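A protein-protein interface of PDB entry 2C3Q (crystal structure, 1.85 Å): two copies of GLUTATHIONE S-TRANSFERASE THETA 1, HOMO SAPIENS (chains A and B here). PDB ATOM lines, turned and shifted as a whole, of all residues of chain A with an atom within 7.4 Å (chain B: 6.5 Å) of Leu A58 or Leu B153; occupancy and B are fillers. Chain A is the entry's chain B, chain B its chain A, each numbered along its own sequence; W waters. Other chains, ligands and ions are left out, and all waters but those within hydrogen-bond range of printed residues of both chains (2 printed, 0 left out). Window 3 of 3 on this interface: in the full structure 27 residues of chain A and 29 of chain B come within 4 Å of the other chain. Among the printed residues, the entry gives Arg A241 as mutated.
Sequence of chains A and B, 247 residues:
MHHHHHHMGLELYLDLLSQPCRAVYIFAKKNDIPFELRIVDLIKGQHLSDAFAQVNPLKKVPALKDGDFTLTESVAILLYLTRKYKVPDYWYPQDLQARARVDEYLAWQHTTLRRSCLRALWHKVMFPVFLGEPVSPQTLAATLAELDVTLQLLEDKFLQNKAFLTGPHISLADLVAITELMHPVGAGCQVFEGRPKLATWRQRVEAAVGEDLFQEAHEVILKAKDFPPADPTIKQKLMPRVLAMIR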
ATOM      1  N   HIS A  47     -20.231  -3.249  16.538  1.00  0.00           N
ATOM      2  CA  HIS A  47     -19.969  -4.199  17.633  1.00  0.00           C
ATOM      3  C   HIS A  47     -18.634  -3.912  18.321  1.00  0.00           C
ATOM      4  O   HIS A  47     -18.402  -4.389  19.423  1.00  0.00           O
ATOM      5  CB  HIS A  47     -20.039  -5.645  17.113  1.00  0.00           C
ATOM      6  CG  HIS A  47     -18.998  -5.973  16.096  1.00  0.00           C
ATOM      7  ND1 HIS A  47     -19.054  -5.512  14.796  1.00  0.00           N
ATOM      8  CD2 HIS A  47     -17.877  -6.722  16.183  1.00  0.00           C
ATOM      9  CE1 HIS A  47     -18.015  -5.970  14.127  1.00  0.00           C
ATOM     10  NE2 HIS A  47     -17.279  -6.697  14.948  1.00  0.00           N
ATOM     11  N   LEU A  48     -17.780  -3.128  17.663  1.00  0.00           N
ATOM     12  CA  LEU A  48     -16.479  -2.734  18.182  1.00  0.00           C
ATOM     13  C   LEU A  48     -16.509  -1.375  18.920  1.00  0.00           C
ATOM     14  O   LEU A  48     -15.467  -0.904  19.402  1.00  0.00           O
ATOM     15  CB  LEU A  48     -15.444  -2.721  17.040  1.00  0.00           C
ATOM     16  CG  LEU A  48     -15.160  -4.036  16.299  1.00  0.00           C
ATOM     17  CD1 LEU A  48     -14.108  -3.813  15.242  1.00  0.00           C
ATOM     18  CD2 LEU A  48     -14.713  -5.161  17.238  1.00  0.00           C
ATOM     19  N   PHE A  52     -21.324  -0.710  22.544  1.00  0.00           N
ATOM     20  CA  PHE A  52     -21.690  -2.146  22.469  1.00  0.00           C
ATOM     21  C   PHE A  52     -20.842  -2.961  23.437  1.00  0.00           C
ATOM     22  O   PHE A  52     -21.349  -3.924  24.023  1.00  0.00           O
ATOM     23  CB  PHE A  52     -21.587  -2.768  21.067  1.00  0.00           C
ATOM     24  CG  PHE A  52     -22.085  -4.189  21.044  1.00  0.00           C
ATOM     25  CD1 PHE A  52     -23.447  -4.454  21.245  1.00  0.00           C
ATOM     26  CD2 PHE A  52     -21.197  -5.263  20.936  1.00  0.00           C
ATOM     27  CE1 PHE A  52     -23.917  -5.760  21.284  1.00  0.00           C
ATOM     28  CE2 PHE A  52     -21.662  -6.581  20.958  1.00  0.00           C
ATOM     29  CZ  PHE A  52     -23.016  -6.826  21.140  1.00  0.00           C
ATOM     30  N   ALA A  53     -19.578  -2.570  23.618  1.00  0.00           N
ATOM     31  CA  ALA A  53     -18.665  -3.229  24.573  1.00  0.00           C
ATOM     32  C   ALA A  53     -19.213  -3.238  26.024  1.00  0.00           C
ATOM     33  O   ALA A  53     -18.882  -4.133  26.803  1.00  0.00           O
ATOM     34  CB  ALA A  53     -17.273  -2.597  24.509  1.00  0.00           C
ATOM     35  N   VAL A  55     -22.540  -3.562  26.649  1.00  0.00           N
ATOM     36  CA  VAL A  55     -23.543  -4.630  26.611  1.00  0.00           C
ATOM     37  C   VAL A  55     -22.790  -5.973  26.654  1.00  0.00           C
ATOM     38  O   VAL A  55     -22.918  -6.722  27.630  1.00  0.00           O
ATOM     39  CB  VAL A  55     -24.508  -4.515  25.391  1.00  0.00           C
ATOM     40  CG1 VAL A  55     -25.490  -5.683  25.347  1.00  0.00           C
ATOM     41  CG2 VAL A  55     -25.260  -3.172  25.397  1.00  0.00           C
ATOM     42  N   ASN A  56     -21.976  -6.238  25.628  1.00  0.00           N
ATOM     43  CA  ASN A  56     -21.173  -7.457  25.556  1.00  0.00           C
ATOM     44  C   ASN A  56     -19.685  -7.134  25.366  1.00  0.00           C
ATOM     45  O   ASN A  56     -19.265  -6.832  24.239  1.00  0.00           O
ATOM     46  CB  ASN A  56     -21.696  -8.413  24.456  1.00  0.00           C
ATOM     47  CG  ASN A  56     -20.881  -9.709  24.343  1.00  0.00           C
ATOM     48  OD1 ASN A  56     -20.085 -10.056  25.223  1.00  0.00           O
ATOM     49  ND2 ASN A  56     -21.116 -10.457  23.268  1.00  0.00           N
ATOM     50  N   PRO A  57     -18.870  -7.289  26.446  1.00  0.00           N
ATOM     51  CA  PRO A  57     -17.407  -7.045  26.433  1.00  0.00           C
ATOM     52  C   PRO A  57     -16.638  -7.914  25.432  1.00  0.00           C
ATOM     53  O   PRO A  57     -15.563  -7.517  25.005  1.00  0.00           O
ATOM     54  CB  PRO A  57     -16.981  -7.392  27.862  1.00  0.00           C
ATOM     55  CG  PRO A  57     -18.233  -7.251  28.672  1.00  0.00           C
ATOM     56  CD  PRO A  57     -19.307  -7.750  27.780  1.00  0.00           C
ATOM     57  N   LEU A  58     -17.220  -9.044  25.023  1.00  0.00           N
ATOM     58  CA  LEU A  58     -16.616  -9.947  24.030  1.00  0.00           C
ATOM     59  C   LEU A  58     -16.768  -9.425  22.596  1.00  0.00           C
ATOM     60  O   LEU A  58     -16.187 -10.001  21.665  1.00  0.00           O
ATOM     61  CB  LEU A  58     -17.199 -11.376  24.146  1.00  0.00           C
ATOM     62  CG  LEU A  58     -17.100 -12.137  25.478  1.00  0.00           C
ATOM     63  CD1 LEU A  58     -17.836 -13.450  25.351  1.00  0.00           C
ATOM     64  CD2 LEU A  58     -15.661 -12.391  25.919  1.00  0.00           C
ATOM     65  N   LYS A  59     -17.572  -8.364  22.441  1.00  0.00           N
ATOM     66  CA  LYS A  59     -17.815  -7.609  21.187  1.00  0.00           C
ATOM     67  C   LYS A  59     -18.330  -8.497  20.035  1.00  0.00           C
ATOM     68  O   LYS A  59     -17.862  -8.438  18.896  1.00  0.00           O
ATOM     69  CB  LYS A  59     -16.552  -6.803  20.794  1.00  0.00           C
ATOM     70  CG  LYS A  59     -16.321  -5.586  21.719  1.00  0.00           C
ATOM     71  CD  LYS A  59     -15.260  -4.652  21.151  1.00  0.00           C
ATOM     72  CE  LYS A  59     -13.864  -4.950  21.620  1.00  0.00           C
ATOM     73  NZ  LYS A  59     -13.702  -4.267  22.929  1.00  0.00           N
ATOM     74  N   LYS A  60     -19.283  -9.352  20.393  1.00  0.00           N
ATOM     75  CA  LYS A  60     -19.908 -10.283  19.473  1.00  0.00           C
ATOM     76  C   LYS A  60     -21.423 -10.272  19.644  1.00  0.00           C
ATOM     77  O   LYS A  60     -21.944  -9.869  20.683  1.00  0.00           O
ATOM     78  CB  LYS A  60     -19.331 -11.692  19.679  1.00  0.00           C
ATOM     79  CG  LYS A  60     -17.889 -11.854  19.195  1.00  0.00           C
ATOM     80  CD  LYS A  60     -17.264 -13.153  19.601  1.00  0.00           C
ATOM     81  CE  LYS A  60     -15.914 -13.299  18.950  1.00  0.00           C
ATOM     82  NZ  LYS A  60     -15.226 -14.494  19.475  1.00  0.00           N
ATOM     83  N   VAL A  61     -22.112 -10.724  18.600  1.00  0.00           N
ATOM     84  CA  VAL A  61     -23.562 -10.865  18.560  1.00  0.00           C
ATOM     85  C   VAL A  61     -23.927 -12.355  18.296  1.00  0.00           C
ATOM     86  O   VAL A  61     -23.157 -13.050  17.614  1.00  0.00           O
ATOM     87  CB  VAL A  61     -24.248  -9.886  17.523  1.00  0.00           C
ATOM     88  CG1 VAL A  61     -24.180  -8.435  17.981  1.00  0.00           C
ATOM     89  CG2 VAL A  61     -23.655 -10.030  16.116  1.00  0.00           C
ATOM     90  N   THR A  72     -24.927 -14.093  26.672  1.00  0.00           N
ATOM     91  CA  THR A  72     -24.293 -14.318  25.366  1.00  0.00           C
ATOM     92  C   THR A  72     -24.527 -15.800  24.975  1.00  0.00           C
ATOM     93  O   THR A  72     -25.116 -16.561  25.751  1.00  0.00           O
ATOM     94  CB  THR A  72     -22.783 -13.918  25.331  1.00  0.00           C
ATOM     95  OG1 THR A  72     -22.008 -14.856  26.091  1.00  0.00           O
ATOM     96  CG2 THR A  72     -22.562 -12.506  25.879  1.00  0.00           C
ATOM     97  N   GLU A  73     -24.108 -16.163  23.759  1.00  0.00           N
ATOM     98  CA  GLU A  73     -24.182 -17.516  23.132  1.00  0.00           C
ATOM     99  C   GLU A  73     -25.567 -17.826  22.655  1.00  0.00           C
ATOM    100  O   GLU A  73     -26.495 -17.904  23.448  1.00  0.00           O
ATOM    101  CB  GLU A  73     -23.709 -18.655  24.059  1.00  0.00           C
ATOM    102  CG  GLU A  73     -22.210 -18.596  24.387  1.00  0.00           C
ATOM    103  CD  GLU A  73     -21.311 -18.820  23.162  1.00  0.00           C
ATOM    104  OE1 GLU A  73     -21.638 -19.632  22.263  1.00  0.00           O
ATOM    105  OE2 GLU A  73     -20.262 -18.192  23.126  1.00  0.00           O
ATOM    106  N   ARG A 241     -10.140  -9.739  14.041  1.00  0.00           N
ATOM    107  CA  ARG A 241     -11.383 -10.282  14.558  1.00  0.00           C
ATOM    108  C   ARG A 241     -11.889 -11.381  13.646  1.00  0.00           C
ATOM    109  O   ARG A 241     -12.276 -12.443  14.122  1.00  0.00           O
ATOM    110  CB  ARG A 241     -12.449  -9.195  14.662  1.00  0.00           C
ATOM    111  CG  ARG A 241     -12.140  -7.958  15.519  1.00  0.00           C
ATOM    112  CD  ARG A 241     -12.163  -8.198  17.021  1.00  0.00           C
ATOM    113  NE  ARG A 241     -13.431  -8.770  17.484  1.00  0.00           N
ATOM    114  CZ  ARG A 241     -13.761  -8.961  18.757  1.00  0.00           C
ATOM    115  NH1 ARG A 241     -12.936  -8.595  19.733  1.00  0.00           N
ATOM    116  NH2 ARG A 241     -14.935  -9.501  19.054  1.00  0.00           N
ATOM    117  N   ARG A 247     -10.582 -19.488  11.899  1.00  0.00           N
ATOM    118  CA  ARG A 247      -9.729 -20.662  12.291  1.00  0.00           C
ATOM    119  C   ARG A 247     -10.404 -22.083  12.420  1.00  0.00           C
ATOM    120  O   ARG A 247     -11.567 -22.265  12.832  1.00  0.00           O
ATOM    121  CB  ARG A 247      -9.008 -20.308  13.603  1.00  0.00           C
ATOM    122  CG  ARG A 247      -9.939 -20.311  14.814  1.00  0.00           C
ATOM    123  CD  ARG A 247      -9.313 -19.755  16.024  1.00  0.00           C
ATOM    124  NE  ARG A 247     -10.160 -19.995  17.190  1.00  0.00           N
ATOM    125  CZ  ARG A 247     -10.070 -19.296  18.319  1.00  0.00           C
ATOM    126  NH1 ARG A 247      -9.218 -18.277  18.401  1.00  0.00           N
ATOM    127  NH2 ARG A 247     -10.867 -19.571  19.341  1.00  0.00           N
ATOM    128  OXT ARG A 247      -9.788 -23.118  12.084  1.00  0.00           O
ATOM    129  N   GLU B 104     -24.321 -20.896  28.872  1.00  0.00           N
ATOM    130  CA  GLU B 104     -23.409 -19.903  28.299  1.00  0.00           C
ATOM    131  C   GLU B 104     -21.976 -20.421  28.284  1.00  0.00           C
ATOM    132  O   GLU B 104     -21.323 -20.336  27.250  1.00  0.00           O
ATOM    133  CB  GLU B 104     -23.490 -18.576  29.064  1.00  0.00           C
ATOM    134  CG  GLU B 104     -22.707 -17.429  28.423  1.00  0.00           C
ATOM    135  CD  GLU B 104     -22.761 -16.134  29.241  1.00  0.00           C
ATOM    136  OE1 GLU B 104     -22.705 -16.179  30.492  1.00  0.00           O
ATOM    137  OE2 GLU B 104     -22.880 -15.062  28.617  1.00  0.00           O
ATOM    138  N   TRP B 108     -19.893 -21.653  24.869  1.00  0.00           N
ATOM    139  CA  TRP B 108     -18.667 -20.931  24.557  1.00  0.00           C
ATOM    140  C   TRP B 108     -17.409 -21.800  24.398  1.00  0.00           C
ATOM    141  O   TRP B 108     -16.658 -21.628  23.433  1.00  0.00           O
ATOM    142  CB  TRP B 108     -18.445 -19.888  25.676  1.00  0.00           C
ATOM    143  CG  TRP B 108     -17.175 -19.088  25.558  1.00  0.00           C
ATOM    144  CD1 TRP B 108     -16.975 -17.955  24.808  1.00  0.00           C
ATOM    145  CD2 TRP B 108     -15.931 -19.360  26.221  1.00  0.00           C
ATOM    146  NE1 TRP B 108     -15.683 -17.516  24.967  1.00  0.00           N
ATOM    147  CE2 TRP B 108     -15.022 -18.356  25.829  1.00  0.00           C
ATOM    148  CE3 TRP B 108     -15.507 -20.353  27.124  1.00  0.00           C
ATOM    149  CZ2 TRP B 108     -13.698 -18.316  26.293  1.00  0.00           C
ATOM    150  CZ3 TRP B 108     -14.194 -20.319  27.595  1.00  0.00           C
ATOM    151  CH2 TRP B 108     -13.299 -19.310  27.160  1.00  0.00           C
ATOM    152  N   THR B 112     -13.341 -22.419  21.806  1.00  0.00           N
ATOM    153  CA  THR B 112     -12.379 -21.518  22.428  1.00  0.00           C
ATOM    154  C   THR B 112     -11.455 -22.324  23.344  1.00  0.00           C
ATOM    155  O   THR B 112     -10.422 -22.781  22.878  1.00  0.00           O
ATOM    156  CB  THR B 112     -13.114 -20.373  23.172  1.00  0.00           C
ATOM    157  OG1 THR B 112     -13.986 -20.930  24.148  1.00  0.00           O
ATOM    158  CG2 THR B 112     -13.968 -19.438  22.226  1.00  0.00           C
ATOM    159  N   ASP B 148      -3.251 -18.746  26.171  1.00  0.00           N
ATOM    160  CA  ASP B 148      -3.215 -17.640  27.141  1.00  0.00           C
ATOM    161  C   ASP B 148      -4.408 -16.684  26.991  1.00  0.00           C
ATOM    162  O   ASP B 148      -4.942 -16.221  28.002  1.00  0.00           O
ATOM    163  CB  ASP B 148      -1.901 -16.846  27.048  1.00  0.00           C
ATOM    164  CG  ASP B 148      -0.704 -17.595  27.631  1.00  0.00           C
ATOM    165  OD1 ASP B 148      -0.838 -18.696  28.251  1.00  0.00           O
ATOM    166  OD2 ASP B 148       0.412 -17.057  27.451  1.00  0.00           O
ATOM    167  N   VAL B 149      -4.832 -16.424  25.746  1.00  0.00           N
ATOM    168  CA  VAL B 149      -6.019 -15.598  25.470  1.00  0.00           C
ATOM    169  C   VAL B 149      -7.262 -16.265  26.079  1.00  0.00           C
ATOM    170  O   VAL B 149      -8.047 -15.602  26.777  1.00  0.00           O
ATOM    171  CB  VAL B 149      -6.187 -15.310  23.939  1.00  0.00           C
ATOM    172  CG1 VAL B 149      -7.576 -14.783  23.586  1.00  0.00           C
ATOM    173  CG2 VAL B 149      -5.121 -14.326  23.438  1.00  0.00           C
ATOM    174  N   THR B 150      -7.398 -17.581  25.878  1.00  0.00           N
ATOM    175  CA  THR B 150      -8.567 -18.295  26.422  1.00  0.00           C
ATOM    176  C   THR B 150      -8.537 -18.352  27.952  1.00  0.00           C
ATOM    177  O   THR B 150      -9.585 -18.332  28.573  1.00  0.00           O
ATOM    178  CB  THR B 150      -8.742 -19.724  25.810  1.00  0.00           C
ATOM    179  OG1 THR B 150      -7.590 -20.520  26.090  1.00  0.00           O
ATOM    180  CG2 THR B 150      -8.895 -19.609  24.346  1.00  0.00           C
ATOM    181  N   LEU B 151      -7.342 -18.462  28.545  1.00  0.00           N
ATOM    182  CA  LEU B 151      -7.208 -18.501  30.007  1.00  0.00           C
ATOM    183  C   LEU B 151      -7.601 -17.151  30.629  1.00  0.00           C
ATOM    184  O   LEU B 151      -8.193 -17.125  31.724  1.00  0.00           O
ATOM    185  CB  LEU B 151      -5.793 -18.931  30.439  1.00  0.00           C
ATOM    186  CG  LEU B 151      -5.475 -20.433  30.269  1.00  0.00           C
ATOM    187  CD1 LEU B 151      -3.987 -20.729  30.423  1.00  0.00           C
ATOM    188  CD2 LEU B 151      -6.254 -21.241  31.260  1.00  0.00           C
ATOM    189  N   GLN B 152      -7.284 -16.061  29.928  1.00  0.00           N
ATOM    190  CA  GLN B 152      -7.647 -14.707  30.352  1.00  0.00           C
ATOM    191  C   GLN B 152      -9.159 -14.509  30.249  1.00  0.00           C
ATOM    192  O   GLN B 152      -9.754 -13.926  31.139  1.00  0.00           O
ATOM    193  CB  GLN B 152      -6.908 -13.645  29.532  1.00  0.00           C
ATOM    194  CG  GLN B 152      -6.983 -12.229  30.121  1.00  0.00           C
ATOM    195  CD  GLN B 152      -6.384 -12.146  31.543  1.00  0.00           C
ATOM    196  OE1 GLN B 152      -5.335 -12.730  31.835  1.00  0.00           O
ATOM    197  NE2 GLN B 152      -7.057 -11.424  32.422  1.00  0.00           N
ATOM    198  N   LEU B 153      -9.757 -14.999  29.159  1.00  0.00           N
ATOM    199  CA  LEU B 153     -11.213 -14.953  28.969  1.00  0.00           C
ATOM    200  C   LEU B 153     -11.939 -15.801  30.024  1.00  0.00           C
ATOM    201  O   LEU B 153     -12.960 -15.348  30.531  1.00  0.00           O
ATOM    202  CB  LEU B 153     -11.611 -15.377  27.547  1.00  0.00           C
ATOM    203  CG  LEU B 153     -11.264 -14.451  26.367  1.00  0.00           C
ATOM    204  CD1 LEU B 153     -11.603 -15.116  25.042  1.00  0.00           C
ATOM    205  CD2 LEU B 153     -11.971 -13.113  26.482  1.00  0.00           C
ATOM    206  N   LEU B 154     -11.398 -16.981  30.368  1.00  0.00           N
ATOM    207  CA  LEU B 154     -11.938 -17.820  31.448  1.00  0.00           C
ATOM    208  C   LEU B 154     -12.051 -17.025  32.775  1.00  0.00           C
ATOM    209  O   LEU B 154     -13.116 -16.986  33.402  1.00  0.00           O
ATOM    210  CB  LEU B 154     -11.095 -19.092  31.657  1.00  0.00           C
ATOM    211  CG  LEU B 154     -11.644 -20.161  32.624  1.00  0.00           C
ATOM    212  CD1 LEU B 154     -13.025 -20.704  32.169  1.00  0.00           C
ATOM    213  CD2 LEU B 154     -10.658 -21.318  32.825  1.00  0.00           C
ATOM    214  N   GLU B 155     -10.955 -16.359  33.144  1.00  0.00           N
ATOM    215  CA  GLU B 155     -10.907 -15.498  34.321  1.00  0.00           C
ATOM    216  C   GLU B 155     -11.815 -14.266  34.235  1.00  0.00           C
ATOM    217  O   GLU B 155     -12.593 -14.039  35.147  1.00  0.00           O
ATOM    218  CB  GLU B 155      -9.479 -14.988  34.583  1.00  0.00           C
ATOM    219  CG  GLU B 155      -8.561 -15.864  35.466  1.00  0.00           C
ATOM    220  CD  GLU B 155      -7.336 -15.087  36.044  1.00  0.00           C
ATOM    221  OE1 GLU B 155      -7.166 -13.901  35.694  1.00  0.00           O
ATOM    222  OE2 GLU B 155      -6.543 -15.635  36.860  1.00  0.00           O
ATOM    223  N   ASP B 156     -11.734 -13.515  33.133  1.00  0.00           N
ATOM    224  CA  ASP B 156     -12.440 -12.213  32.990  1.00  0.00           C
ATOM    225  C   ASP B 156     -13.920 -12.264  32.614  1.00  0.00           C
ATOM    226  O   ASP B 156     -14.673 -11.383  33.032  1.00  0.00           O
ATOM    227  CB  ASP B 156     -11.701 -11.339  31.943  1.00  0.00           C
ATOM    228  CG  ASP B 156     -10.273 -10.934  32.388  1.00  0.00           C
ATOM    229  OD1 ASP B 156      -9.887 -11.138  33.571  1.00  0.00           O
ATOM    230  OD2 ASP B 156      -9.519 -10.401  31.535  1.00  0.00           O
ATOM    231  N   LYS B 157     -14.325 -13.229  31.790  1.00  0.00           N
ATOM    232  CA  LYS B 157     -15.725 -13.338  31.374  1.00  0.00           C
ATOM    233  C   LYS B 157     -16.495 -14.209  32.347  1.00  0.00           C
ATOM    234  O   LYS B 157     -17.623 -13.881  32.694  1.00  0.00           O
ATOM    235  CB  LYS B 157     -15.851 -13.893  29.931  1.00  0.00           C
ATOM    236  CG  LYS B 157     -17.175 -13.608  29.172  1.00  0.00           C
ATOM    237  CD  LYS B 157     -18.235 -14.646  29.343  1.00  0.00           C
ATOM    238  CE  LYS B 157     -19.572 -14.280  28.719  1.00  0.00           C
ATOM    239  NZ  LYS B 157     -20.321 -13.309  29.580  1.00  0.00           N
ATOM    240  N   PHE B 158     -15.884 -15.296  32.821  1.00  0.00           N
ATOM    241  CA  PHE B 158     -16.653 -16.274  33.613  1.00  0.00           C
ATOM    242  C   PHE B 158     -16.363 -16.225  35.103  1.00  0.00           C
ATOM    243  O   PHE B 158     -17.254 -15.886  35.847  1.00  0.00           O
ATOM    244  CB  PHE B 158     -16.435 -17.692  33.063  1.00  0.00           C
ATOM    245  CG  PHE B 158     -16.945 -17.855  31.673  1.00  0.00           C
ATOM    246  CD1 PHE B 158     -18.305 -18.102  31.441  1.00  0.00           C
ATOM    247  CD2 PHE B 158     -16.081 -17.727  30.586  1.00  0.00           C
ATOM    248  CE1 PHE B 158     -18.789 -18.249  30.126  1.00  0.00           C
ATOM    249  CE2 PHE B 158     -16.547 -17.860  29.277  1.00  0.00           C
ATOM    250  CZ  PHE B 158     -17.902 -18.146  29.043  1.00  0.00           C
ATOM    251  N   LEU B 159     -15.155 -16.618  35.522  1.00  0.00           N
ATOM    252  CA  LEU B 159     -14.845 -16.787  36.957  1.00  0.00           C
ATOM    253  C   LEU B 159     -14.955 -15.481  37.751  1.00  0.00           C
ATOM    254  O   LEU B 159     -15.609 -15.478  38.803  1.00  0.00           O
ATOM    255  CB  LEU B 159     -13.449 -17.421  37.162  1.00  0.00           C
ATOM    256  CG  LEU B 159     -13.025 -17.709  38.623  1.00  0.00           C
ATOM    257  CD1 LEU B 159     -13.922 -18.731  39.356  1.00  0.00           C
ATOM    258  CD2 LEU B 159     -11.584 -18.183  38.676  1.00  0.00           C
HETATM  259  O   HOH W   1     -20.111 -11.076  27.782  1.00  0.00           O
HETATM  260  O   HOH W   2      -9.027 -21.689  20.472  1.00  0.00           O
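OE2 of Glu B104 lies within salt-bridge range of NZ of Lys B157, 3.2 Å away. The backbone carbonyl oxygen (O) of Trp B108 lies within hydrogen-bond range of the side-chain hydroxyl (OG1) of Thr B112, at 2.9 Å. N of Leu A58 sits at hydrogen-bond distance from OD1 of Asn A56. O of Leu A58 sits at hydrogen-bond distance from NH2 of Arg A241.
The side-chain hydroxyl (OG1) of Thr A72 sits at hydrogen-bond distance from the side-chain carboxylate (OE2) of Glu B104 (2.7 Å).
Of the 15 printed residues of chain B, 5 touch a printed residue of chain A. Printed residues of chain B that touch a printed residue of chain A: Glu B104, Trp B108, Thr B112, Leu B153 and Lys B157. Hydrophobic or aromatic side chains of chain B within 4 Å of the printed part of chain A: Trp B108 and Leu B153. Among the printed residues, no Asp or Glu carboxylate lies within 4 Å of a Lys or Arg side-chain nitrogen of the other chain.
No position is printed for both chains.
Water W1 lies within hydrogen-bond range of OD1 of Asn A56 (2.8 Å) and NZ of Lys B157 (2.9 Å). Water W2 lies within hydrogen-bond range of O of Thr B112 (3.0 Å) and NH2 of Arg A247 (3.0 Å).
Among the printed residues, pairs that only touch across the chains: Glu A73 with Glu B104 (3.5 Å), Glu A73 with Trp B108 (3.5 Å), Thr A72 with Lys B157 (3.6 Å), Leu A58 with Lys B157 (3.8 Å), Leu A58 with Leu B153 (3.8 Å) and Arg A247 with Thr B112 (3.95 Å).
Of the printed residues of chain B, Leu A58 touches Leu B153 and Lys B157. Of chain A, only Leu A58 (3.8 Å) comes within 4 Å of Leu B153. Of the printed residues of chain A, Trp B108 touches Glu A73. Of the printed residues of chain A, Glu B104 touches Thr A72 and Glu A73. Leu B151 touches none of the printed residues of chain A. Val B149 touches none of the printed residues of chain A. The nearest residue of chain B that does not touch Leu A58 is Trp B108 (4.6 Å). The nearest printed residue of chain A that does not touch Glu B104 is Leu A58 (6.2 Å).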
